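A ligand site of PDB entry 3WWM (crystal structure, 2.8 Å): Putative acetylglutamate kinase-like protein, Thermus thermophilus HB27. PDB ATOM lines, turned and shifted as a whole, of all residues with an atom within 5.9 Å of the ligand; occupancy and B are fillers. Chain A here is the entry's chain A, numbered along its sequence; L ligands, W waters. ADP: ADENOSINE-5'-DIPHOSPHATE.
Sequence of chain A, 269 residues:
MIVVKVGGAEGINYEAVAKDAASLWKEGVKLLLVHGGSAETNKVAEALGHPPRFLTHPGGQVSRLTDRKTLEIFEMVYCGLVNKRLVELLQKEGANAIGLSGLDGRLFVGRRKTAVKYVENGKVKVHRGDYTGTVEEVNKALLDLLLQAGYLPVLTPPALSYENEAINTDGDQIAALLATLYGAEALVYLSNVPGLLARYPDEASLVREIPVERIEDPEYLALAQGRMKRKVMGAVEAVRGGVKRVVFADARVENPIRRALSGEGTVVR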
ATOM      1  N   LYS A   5     -14.017  -3.555  -1.404  1.00  0.00           N
ATOM      2  CA  LYS A   5     -12.690  -4.014  -1.815  1.00  0.00           C
ATOM      3  C   LYS A   5     -12.079  -3.010  -2.784  1.00  0.00           C
ATOM      4  O   LYS A   5     -12.609  -2.798  -3.872  1.00  0.00           O
ATOM      5  CB  LYS A   5     -12.763  -5.376  -2.494  1.00  0.00           C
ATOM      6  CG  LYS A   5     -11.469  -5.844  -3.140  1.00  0.00           C
ATOM      7  CD  LYS A   5     -10.340  -5.991  -2.126  1.00  0.00           C
ATOM      8  CE  LYS A   5      -9.146  -6.765  -2.690  1.00  0.00           C
ATOM      9  NZ  LYS A   5      -8.181  -5.897  -3.419  1.00  0.00           N
ATOM     10  N   VAL A   6     -10.965  -2.389  -2.390  1.00  0.00           N
ATOM     11  CA  VAL A   6     -10.216  -1.507  -3.267  1.00  0.00           C
ATOM     12  C   VAL A   6      -9.136  -2.331  -3.960  1.00  0.00           C
ATOM     13  O   VAL A   6      -8.358  -3.000  -3.297  1.00  0.00           O
ATOM     14  CB  VAL A   6      -9.533  -0.384  -2.483  1.00  0.00           C
ATOM     15  CG1 VAL A   6      -8.956   0.656  -3.431  1.00  0.00           C
ATOM     16  CG2 VAL A   6     -10.522   0.266  -1.515  1.00  0.00           C
ATOM     17  N   GLY A   7      -9.090  -2.271  -5.281  1.00  0.00           N
ATOM     18  CA  GLY A   7      -8.092  -3.016  -6.051  1.00  0.00           C
ATOM     19  C   GLY A   7      -6.723  -2.393  -5.904  1.00  0.00           C
ATOM     20  O   GLY A   7      -6.583  -1.294  -5.376  1.00  0.00           O
ATOM     21  N   GLY A   8      -5.703  -3.098  -6.385  1.00  0.00           N
ATOM     22  CA  GLY A   8      -4.308  -2.665  -6.288  1.00  0.00           C
ATOM     23  C   GLY A   8      -3.609  -2.419  -7.611  1.00  0.00           C
ATOM     24  O   GLY A   8      -2.374  -2.377  -7.672  1.00  0.00           O
ATOM     25  N   ALA A   9      -4.389  -2.220  -8.679  1.00  0.00           N
ATOM     26  CA  ALA A   9      -3.842  -1.915 -10.003  1.00  0.00           C
ATOM     27  C   ALA A   9      -3.397  -0.459 -10.102  1.00  0.00           C
ATOM     28  O   ALA A   9      -3.504   0.307  -9.140  1.00  0.00           O
ATOM     29  CB  ALA A   9      -4.871  -2.233 -11.081  1.00  0.00           C
ATOM     30  N   HIS A  35      -8.191  -3.691   1.025  1.00  0.00           N
ATOM     31  CA  HIS A  35      -7.385  -3.162  -0.074  1.00  0.00           C
ATOM     32  C   HIS A  35      -6.303  -4.144  -0.502  1.00  0.00           C
ATOM     33  O   HIS A  35      -6.220  -5.260   0.032  1.00  0.00           O
ATOM     34  CB  HIS A  35      -6.766  -1.822   0.324  1.00  0.00           C
ATOM     35  CG  HIS A  35      -5.636  -1.957   1.297  1.00  0.00           C
ATOM     36  ND1 HIS A  35      -5.800  -1.717   2.644  1.00  0.00           N
ATOM     37  CD2 HIS A  35      -4.348  -2.316   1.128  1.00  0.00           C
ATOM     38  CE1 HIS A  35      -4.650  -1.910   3.266  1.00  0.00           C
ATOM     39  NE2 HIS A  35      -3.757  -2.276   2.367  1.00  0.00           N
ATOM     40  N   GLY A  36      -5.488  -3.735  -1.472  1.00  0.00           N
ATOM     41  CA  GLY A  36      -4.344  -4.543  -1.915  1.00  0.00           C
ATOM     42  C   GLY A  36      -3.114  -3.706  -2.184  1.00  0.00           C
ATOM     43  O   GLY A  36      -2.754  -2.847  -1.374  1.00  0.00           O
ATOM     44  N   GLY A  37      -2.476  -3.950  -3.322  1.00  0.00           N
ATOM     45  CA  GLY A  37      -1.292  -3.192  -3.755  1.00  0.00           C
ATOM     46  C   GLY A  37      -0.285  -4.048  -4.509  1.00  0.00           C
ATOM     47  O   GLY A  37       0.897  -4.042  -4.183  1.00  0.00           O
ATOM     48  N   SER A  38      -0.751  -4.773  -5.522  1.00  0.00           N
ATOM     49  CA  SER A  38       0.114  -5.677  -6.289  1.00  0.00           C
ATOM     50  C   SER A  38       0.992  -4.895  -7.247  1.00  0.00           C
ATOM     51  O   SER A  38       2.153  -5.240  -7.448  1.00  0.00           O
ATOM     52  CB  SER A  38      -0.728  -6.704  -7.066  1.00  0.00           C
ATOM     53  OG  SER A  38      -1.784  -6.059  -7.760  1.00  0.00           O
ATOM     54  N   ALA A  39       0.428  -3.846  -7.839  1.00  0.00           N
ATOM     55  CA  ALA A  39       1.185  -2.988  -8.763  1.00  0.00           C
ATOM     56  C   ALA A  39       2.358  -2.305  -8.048  1.00  0.00           C
ATOM     57  O   ALA A  39       3.494  -2.374  -8.500  1.00  0.00           O
ATOM     58  CB  ALA A  39       0.268  -1.944  -9.392  1.00  0.00           C
ATOM     59  N   TYR A  78       1.789  -3.665   1.121  1.00  0.00           N
ATOM     60  CA  TYR A  78       0.370  -3.826   1.458  1.00  0.00           C
ATOM     61  C   TYR A  78       0.131  -3.353   2.889  1.00  0.00           C
ATOM     62  O   TYR A  78      -0.761  -2.543   3.145  1.00  0.00           O
ATOM     63  CB  TYR A  78      -0.070  -5.299   1.383  1.00  0.00           C
ATOM     64  CG  TYR A  78      -0.370  -5.841   0.008  1.00  0.00           C
ATOM     65  CD1 TYR A  78       0.606  -5.889  -0.980  1.00  0.00           C
ATOM     66  CD2 TYR A  78      -1.624  -6.373  -0.284  1.00  0.00           C
ATOM     67  CE1 TYR A  78       0.333  -6.420  -2.230  1.00  0.00           C
ATOM     68  CE2 TYR A  78      -1.910  -6.908  -1.538  1.00  0.00           C
ATOM     69  CZ  TYR A  78      -0.928  -6.926  -2.505  1.00  0.00           C
ATOM     70  OH  TYR A  78      -1.182  -7.444  -3.753  1.00  0.00           O
ATOM     71  N   PRO A 157      -4.444  -8.481   3.299  1.00  0.00           N
ATOM     72  CA  PRO A 157      -3.582  -9.642   3.478  1.00  0.00           C
ATOM     73  C   PRO A 157      -2.191  -9.143   3.842  1.00  0.00           C
ATOM     74  O   PRO A 157      -1.946  -7.938   3.787  1.00  0.00           O
ATOM     75  CB  PRO A 157      -3.607 -10.307   2.104  1.00  0.00           C
ATOM     76  CG  PRO A 157      -3.967  -9.230   1.151  1.00  0.00           C
ATOM     77  CD  PRO A 157      -4.919  -8.363   1.913  1.00  0.00           C
ATOM     78  N   ASP A 170      -5.952 -14.283  -1.785  1.00  0.00           N
ATOM     79  CA  ASP A 170      -6.800 -13.512  -2.687  1.00  0.00           C
ATOM     80  C   ASP A 170      -7.639 -12.488  -1.908  1.00  0.00           C
ATOM     81  O   ASP A 170      -8.571 -12.854  -1.185  1.00  0.00           O
ATOM     82  CB  ASP A 170      -7.689 -14.452  -3.483  1.00  0.00           C
ATOM     83  CG  ASP A 170      -8.418 -13.775  -4.613  1.00  0.00           C
ATOM     84  OD1 ASP A 170      -8.653 -12.545  -4.555  1.00  0.00           O
ATOM     85  OD2 ASP A 170      -8.782 -14.475  -5.585  1.00  0.00           O
ATOM     86  N   GLY A 171      -7.316 -11.213  -2.067  1.00  0.00           N
ATOM     87  CA  GLY A 171      -8.060 -10.143  -1.420  1.00  0.00           C
ATOM     88  C   GLY A 171      -9.528 -10.083  -1.775  1.00  0.00           C
ATOM     89  O   GLY A 171     -10.347  -9.685  -0.949  1.00  0.00           O
ATOM     90  N   ASP A 172      -9.876 -10.460  -3.002  1.00  0.00           N
ATOM     91  CA  ASP A 172     -11.268 -10.455  -3.440  1.00  0.00           C
ATOM     92  C   ASP A 172     -12.069 -11.489  -2.680  1.00  0.00           C
ATOM     93  O   ASP A 172     -13.250 -11.265  -2.381  1.00  0.00           O
ATOM     94  CB  ASP A 172     -11.401 -10.700  -4.951  1.00  0.00           C
ATOM     95  CG  ASP A 172     -10.861  -9.559  -5.791  1.00  0.00           C
ATOM     96  OD1 ASP A 172     -10.875  -8.402  -5.337  1.00  0.00           O
ATOM     97  OD2 ASP A 172     -10.413  -9.810  -6.937  1.00  0.00           O
ATOM     98  N   LEU A 190     -13.832  -2.188  -6.349  1.00  0.00           N
ATOM     99  CA  LEU A 190     -13.343  -1.018  -7.083  1.00  0.00           C
ATOM    100  C   LEU A 190     -12.039  -1.333  -7.804  1.00  0.00           C
ATOM    101  O   LEU A 190     -11.130  -1.958  -7.235  1.00  0.00           O
ATOM    102  CB  LEU A 190     -13.141   0.171  -6.152  1.00  0.00           C
ATOM    103  CG  LEU A 190     -14.353   0.673  -5.381  1.00  0.00           C
ATOM    104  CD1 LEU A 190     -13.976   1.916  -4.598  1.00  0.00           C
ATOM    105  CD2 LEU A 190     -15.525   0.957  -6.308  1.00  0.00           C
ATOM    106  N   SER A 191     -11.966  -0.898  -9.048  1.00  0.00           N
ATOM    107  CA  SER A 191     -10.797  -1.154  -9.876  1.00  0.00           C
ATOM    108  C   SER A 191     -10.655  -0.063 -10.933  1.00  0.00           C
ATOM    109  O   SER A 191     -11.509   0.821 -11.034  1.00  0.00           O
ATOM    110  CB  SER A 191     -10.903  -2.524 -10.539  1.00  0.00           C
ATOM    111  OG  SER A 191      -9.631  -2.938 -11.024  1.00  0.00           O
ATOM    112  N   VAL A 193     -11.242   0.209 -13.987  1.00  0.00           N
ATOM    113  CA  VAL A 193     -12.139   0.102 -15.147  1.00  0.00           C
ATOM    114  C   VAL A 193     -13.544   0.424 -14.660  1.00  0.00           C
ATOM    115  O   VAL A 193     -13.783   0.441 -13.453  1.00  0.00           O
ATOM    116  CB  VAL A 193     -12.092  -1.315 -15.775  1.00  0.00           C
ATOM    117  CG1 VAL A 193     -10.687  -1.637 -16.262  1.00  0.00           C
ATOM    118  CG2 VAL A 193     -12.568  -2.377 -14.804  1.00  0.00           C
ATOM    119  N   LEU A 197     -16.962  -5.954 -18.348  1.00  0.00           N
ATOM    120  CA  LEU A 197     -17.163  -5.497 -19.709  1.00  0.00           C
ATOM    121  C   LEU A 197     -16.891  -6.639 -20.687  1.00  0.00           C
ATOM    122  O   LEU A 197     -16.027  -7.476 -20.444  1.00  0.00           O
ATOM    123  CB  LEU A 197     -16.308  -4.247 -19.975  1.00  0.00           C
ATOM    124  CG  LEU A 197     -14.798  -4.319 -20.223  1.00  0.00           C
ATOM    125  CD1 LEU A 197     -14.234  -2.907 -20.105  1.00  0.00           C
ATOM    126  CD2 LEU A 197     -14.071  -5.257 -19.275  1.00  0.00           C
ATOM    127  N   TYR A 200     -13.185  -5.930 -23.635  1.00  0.00           N
ATOM    128  CA  TYR A 200     -12.150  -5.137 -22.972  1.00  0.00           C
ATOM    129  C   TYR A 200     -11.160  -4.686 -24.050  1.00  0.00           C
ATOM    130  O   TYR A 200     -10.799  -5.489 -24.910  1.00  0.00           O
ATOM    131  CB  TYR A 200     -11.447  -5.980 -21.901  1.00  0.00           C
ATOM    132  CG  TYR A 200     -10.161  -5.385 -21.378  1.00  0.00           C
ATOM    133  CD1 TYR A 200     -10.158  -4.464 -20.339  1.00  0.00           C
ATOM    134  CD2 TYR A 200      -8.923  -5.764 -21.916  1.00  0.00           C
ATOM    135  CE1 TYR A 200      -8.967  -3.926 -19.852  1.00  0.00           C
ATOM    136  CE2 TYR A 200      -7.736  -5.243 -21.446  1.00  0.00           C
ATOM    137  CZ  TYR A 200      -7.763  -4.314 -20.419  1.00  0.00           C
ATOM    138  OH  TYR A 200      -6.576  -3.793 -19.949  1.00  0.00           O
ATOM    139  N   ARG A 227     -12.044 -13.946 -18.993  1.00  0.00           N
ATOM    140  CA  ARG A 227     -10.903 -13.411 -18.238  1.00  0.00           C
ATOM    141  C   ARG A 227     -11.222 -13.309 -16.741  1.00  0.00           C
ATOM    142  O   ARG A 227     -10.504 -13.862 -15.911  1.00  0.00           O
ATOM    143  CB  ARG A 227     -10.503 -12.026 -18.791  1.00  0.00           C
ATOM    144  CG  ARG A 227      -9.062 -11.611 -18.498  1.00  0.00           C
ATOM    145  CD  ARG A 227      -8.084 -12.208 -19.492  1.00  0.00           C
ATOM    146  NE  ARG A 227      -6.955 -11.315 -19.769  1.00  0.00           N
ATOM    147  CZ  ARG A 227      -5.917 -11.122 -18.959  1.00  0.00           C
ATOM    148  NH1 ARG A 227      -5.828 -11.738 -17.790  1.00  0.00           N
ATOM    149  NH2 ARG A 227      -4.949 -10.279 -19.321  1.00  0.00           N
ATOM    150  N   MET A 228     -12.315 -12.616 -16.414  1.00  0.00           N
ATOM    151  CA  MET A 228     -12.735 -12.416 -15.025  1.00  0.00           C
ATOM    152  C   MET A 228     -13.764 -13.475 -14.609  1.00  0.00           C
ATOM    153  O   MET A 228     -14.939 -13.169 -14.470  1.00  0.00           O
ATOM    154  CB  MET A 228     -13.316 -11.004 -14.828  1.00  0.00           C
ATOM    155  CG  MET A 228     -12.496  -9.834 -15.372  1.00  0.00           C
ATOM    156  SD  MET A 228     -12.796  -9.488 -17.124  1.00  0.00           S
ATOM    157  CE  MET A 228     -13.127  -7.725 -17.166  1.00  0.00           C
ATOM    158  N   ARG A 230     -13.081 -15.804 -11.762  1.00  0.00           N
ATOM    159  CA  ARG A 230     -12.955 -15.909 -10.292  1.00  0.00           C
ATOM    160  C   ARG A 230     -13.728 -14.828  -9.538  1.00  0.00           C
ATOM    161  O   ARG A 230     -14.383 -15.114  -8.538  1.00  0.00           O
ATOM    162  CB  ARG A 230     -11.475 -15.910  -9.864  1.00  0.00           C
ATOM    163  CG  ARG A 230     -10.574 -14.898 -10.571  1.00  0.00           C
ATOM    164  CD  ARG A 230      -9.211 -14.792  -9.910  1.00  0.00           C
ATOM    165  NE  ARG A 230      -9.199 -13.849  -8.798  1.00  0.00           N
ATOM    166  CZ  ARG A 230      -9.245 -12.518  -8.910  1.00  0.00           C
ATOM    167  NH1 ARG A 230      -9.239 -11.769  -7.817  1.00  0.00           N
ATOM    168  NH2 ARG A 230      -9.307 -11.936 -10.104  1.00  0.00           N
ATOM    169  N   LYS A 231     -13.656 -13.592 -10.026  1.00  0.00           N
ATOM    170  CA  LYS A 231     -14.419 -12.503  -9.439  1.00  0.00           C
ATOM    171  C   LYS A 231     -15.919 -12.711  -9.644  1.00  0.00           C
ATOM    172  O   LYS A 231     -16.695 -12.611  -8.682  1.00  0.00           O
ATOM    173  CB  LYS A 231     -14.003 -11.143 -10.019  1.00  0.00           C
ATOM    174  CG  LYS A 231     -12.915 -10.395  -9.252  1.00  0.00           C
ATOM    175  CD  LYS A 231     -13.171  -8.895  -9.246  1.00  0.00           C
ATOM    176  CE  LYS A 231     -11.898  -8.067  -9.167  1.00  0.00           C
ATOM    177  NZ  LYS A 231     -12.187  -6.646  -8.841  1.00  0.00           N
HETATM  178  PB  ADP L   1      -4.502  -6.956  -5.084  1.00  0.00           P
HETATM  179  O1B ADP L   1      -4.106  -8.297  -5.640  1.00  0.00           O
HETATM  180  O2B ADP L   1      -5.460  -7.048  -3.925  1.00  0.00           O
HETATM  181  O3B ADP L   1      -3.369  -5.964  -4.957  1.00  0.00           O
HETATM  182  PA  ADP L   1      -6.192  -6.824  -7.414  1.00  0.00           P
HETATM  183  O1A ADP L   1      -6.948  -5.653  -7.999  1.00  0.00           O
HETATM  184  O2A ADP L   1      -6.939  -8.017  -6.908  1.00  0.00           O
HETATM  185  O3A ADP L   1      -5.375  -6.185  -6.180  1.00  0.00           O
HETATM  186  O5' ADP L   1      -5.008  -7.285  -8.418  1.00  0.00           O
HETATM  187  C5' ADP L   1      -4.796  -6.752  -9.741  1.00  0.00           C
HETATM  188  C4' ADP L   1      -5.753  -7.445 -10.715  1.00  0.00           C
HETATM  189  O4' ADP L   1      -6.065  -6.689 -11.897  1.00  0.00           O
HETATM  190  C3' ADP L   1      -5.245  -8.763 -11.282  1.00  0.00           C
HETATM  191  O3' ADP L   1      -5.329  -9.842 -10.350  1.00  0.00           O
HETATM  192  C2' ADP L   1      -6.183  -8.963 -12.457  1.00  0.00           C
HETATM  193  O2' ADP L   1      -7.184  -9.957 -12.201  1.00  0.00           O
HETATM  194  C1' ADP L   1      -6.826  -7.597 -12.687  1.00  0.00           C
HETATM  195  N9  ADP L   1      -6.866  -7.333 -14.159  1.00  0.00           N
HETATM  196  C8  ADP L   1      -5.818  -7.205 -14.995  1.00  0.00           C
HETATM  197  N7  ADP L   1      -6.249  -6.999 -16.270  1.00  0.00           N
HETATM  198  C5  ADP L   1      -7.592  -6.995 -16.258  1.00  0.00           C
HETATM  199  C6  ADP L   1      -8.681  -6.833 -17.246  1.00  0.00           C
HETATM  200  N6  ADP L   1      -8.404  -6.630 -18.540  1.00  0.00           N
HETATM  201  N1  ADP L   1      -9.959  -6.899 -16.817  1.00  0.00           N
HETATM  202  C2  ADP L   1     -10.259  -7.108 -15.517  1.00  0.00           C
HETATM  203  N3  ADP L   1      -9.310  -7.262 -14.564  1.00  0.00           N
HETATM  204  C4  ADP L   1      -7.985  -7.225 -14.862  1.00  0.00           C
HETATM  205  O   HOH W   1      -3.408 -10.324  -2.895  1.00  0.00           O
HETATM  206  O   HOH W   2      -9.438  -6.254  -6.032  1.00  0.00           O
HETATM  207  O   HOH W   3      -5.789  -7.670  -1.195  1.00  0.00           O
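O3B of the ligand is in hydrogen-bond range of N of Gly 37, 2.7 Å away.
An oxygen (O3B) of the ligand lies within hydrogen-bond range of the side-chain hydroxyl (OH) of Tyr 78, at 2.9 Å.
The backbone NH (N) of Ser 38 sits at hydrogen-bond distance from an oxygen (O3B) of the ligand (2.9 Å).
The side-chain hydroxyl (OG) of Ser 38 sits at hydrogen-bond distance from an oxygen (O3B) of the ligand, 3.2 Å away.
An oxygen (O2B) of the ligand is in salt-bridge range of the side-chain amino group (NZ) of Lys 5.
The backbone NH (N) of Gly 8 is in hydrogen-bond range of an oxygen (O3A) of the ligand, 3.1 Å away.
The backbone NH (N) of Ser 38 is in hydrogen-bond range of the side-chain hydroxyl (OH) of Tyr 78 (3.2 Å).
The backbone carbonyl oxygen of Tyr 78 sits at hydrogen-bond distance from a ring nitrogen (NE2) of His 35 (3.1 Å).
The backbone NH of Leu 190 lies within hydrogen-bond range of the backbone carbonyl oxygen of Lys 5, at 2.8 Å.
O of Gly 8 is in hydrogen-bond range of N of Ala 39.
N of Gly 36 sits at hydrogen-bond distance from O of Val 6, 3.5 Å away.
The backbone NH (N) of Gly 7 is in hydrogen-bond range of the backbone carbonyl oxygen (O) of Leu 190, at 2.8 Å.
The guanidinium group (NE) of Arg 230 lies within salt-bridge range of the side-chain carboxylate (OD2) of Asp 170 (3.3 Å).
N of Asp 172 lies within hydrogen-bond range of OD1 of Asp 170, at 2.9 Å.
Merely in contact with the ligand: Tyr 200, Met 228, Gly 36, Gly 7, Arg 230 and Asp 172.
11 residues have an atom within 4 Å of the ligand: Lys 5, Gly 7, Gly 8, Gly 36, Gly 37, Ser 38, Tyr 78, Asp 172, Tyr 200, Met 228 and Arg 230.
Water W3 lies within hydrogen-bond range of the backbone carbonyl oxygen of His 35 (2.7 Å) and an oxygen (O2B) of the ligand (2.8 Å).
Water W2 lies within hydrogen-bond range of OD1 of Asp 172 (2.7 Å), NZ of Lys 5 (2.9 Å) and O2A of the ligand (3.2 Å).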
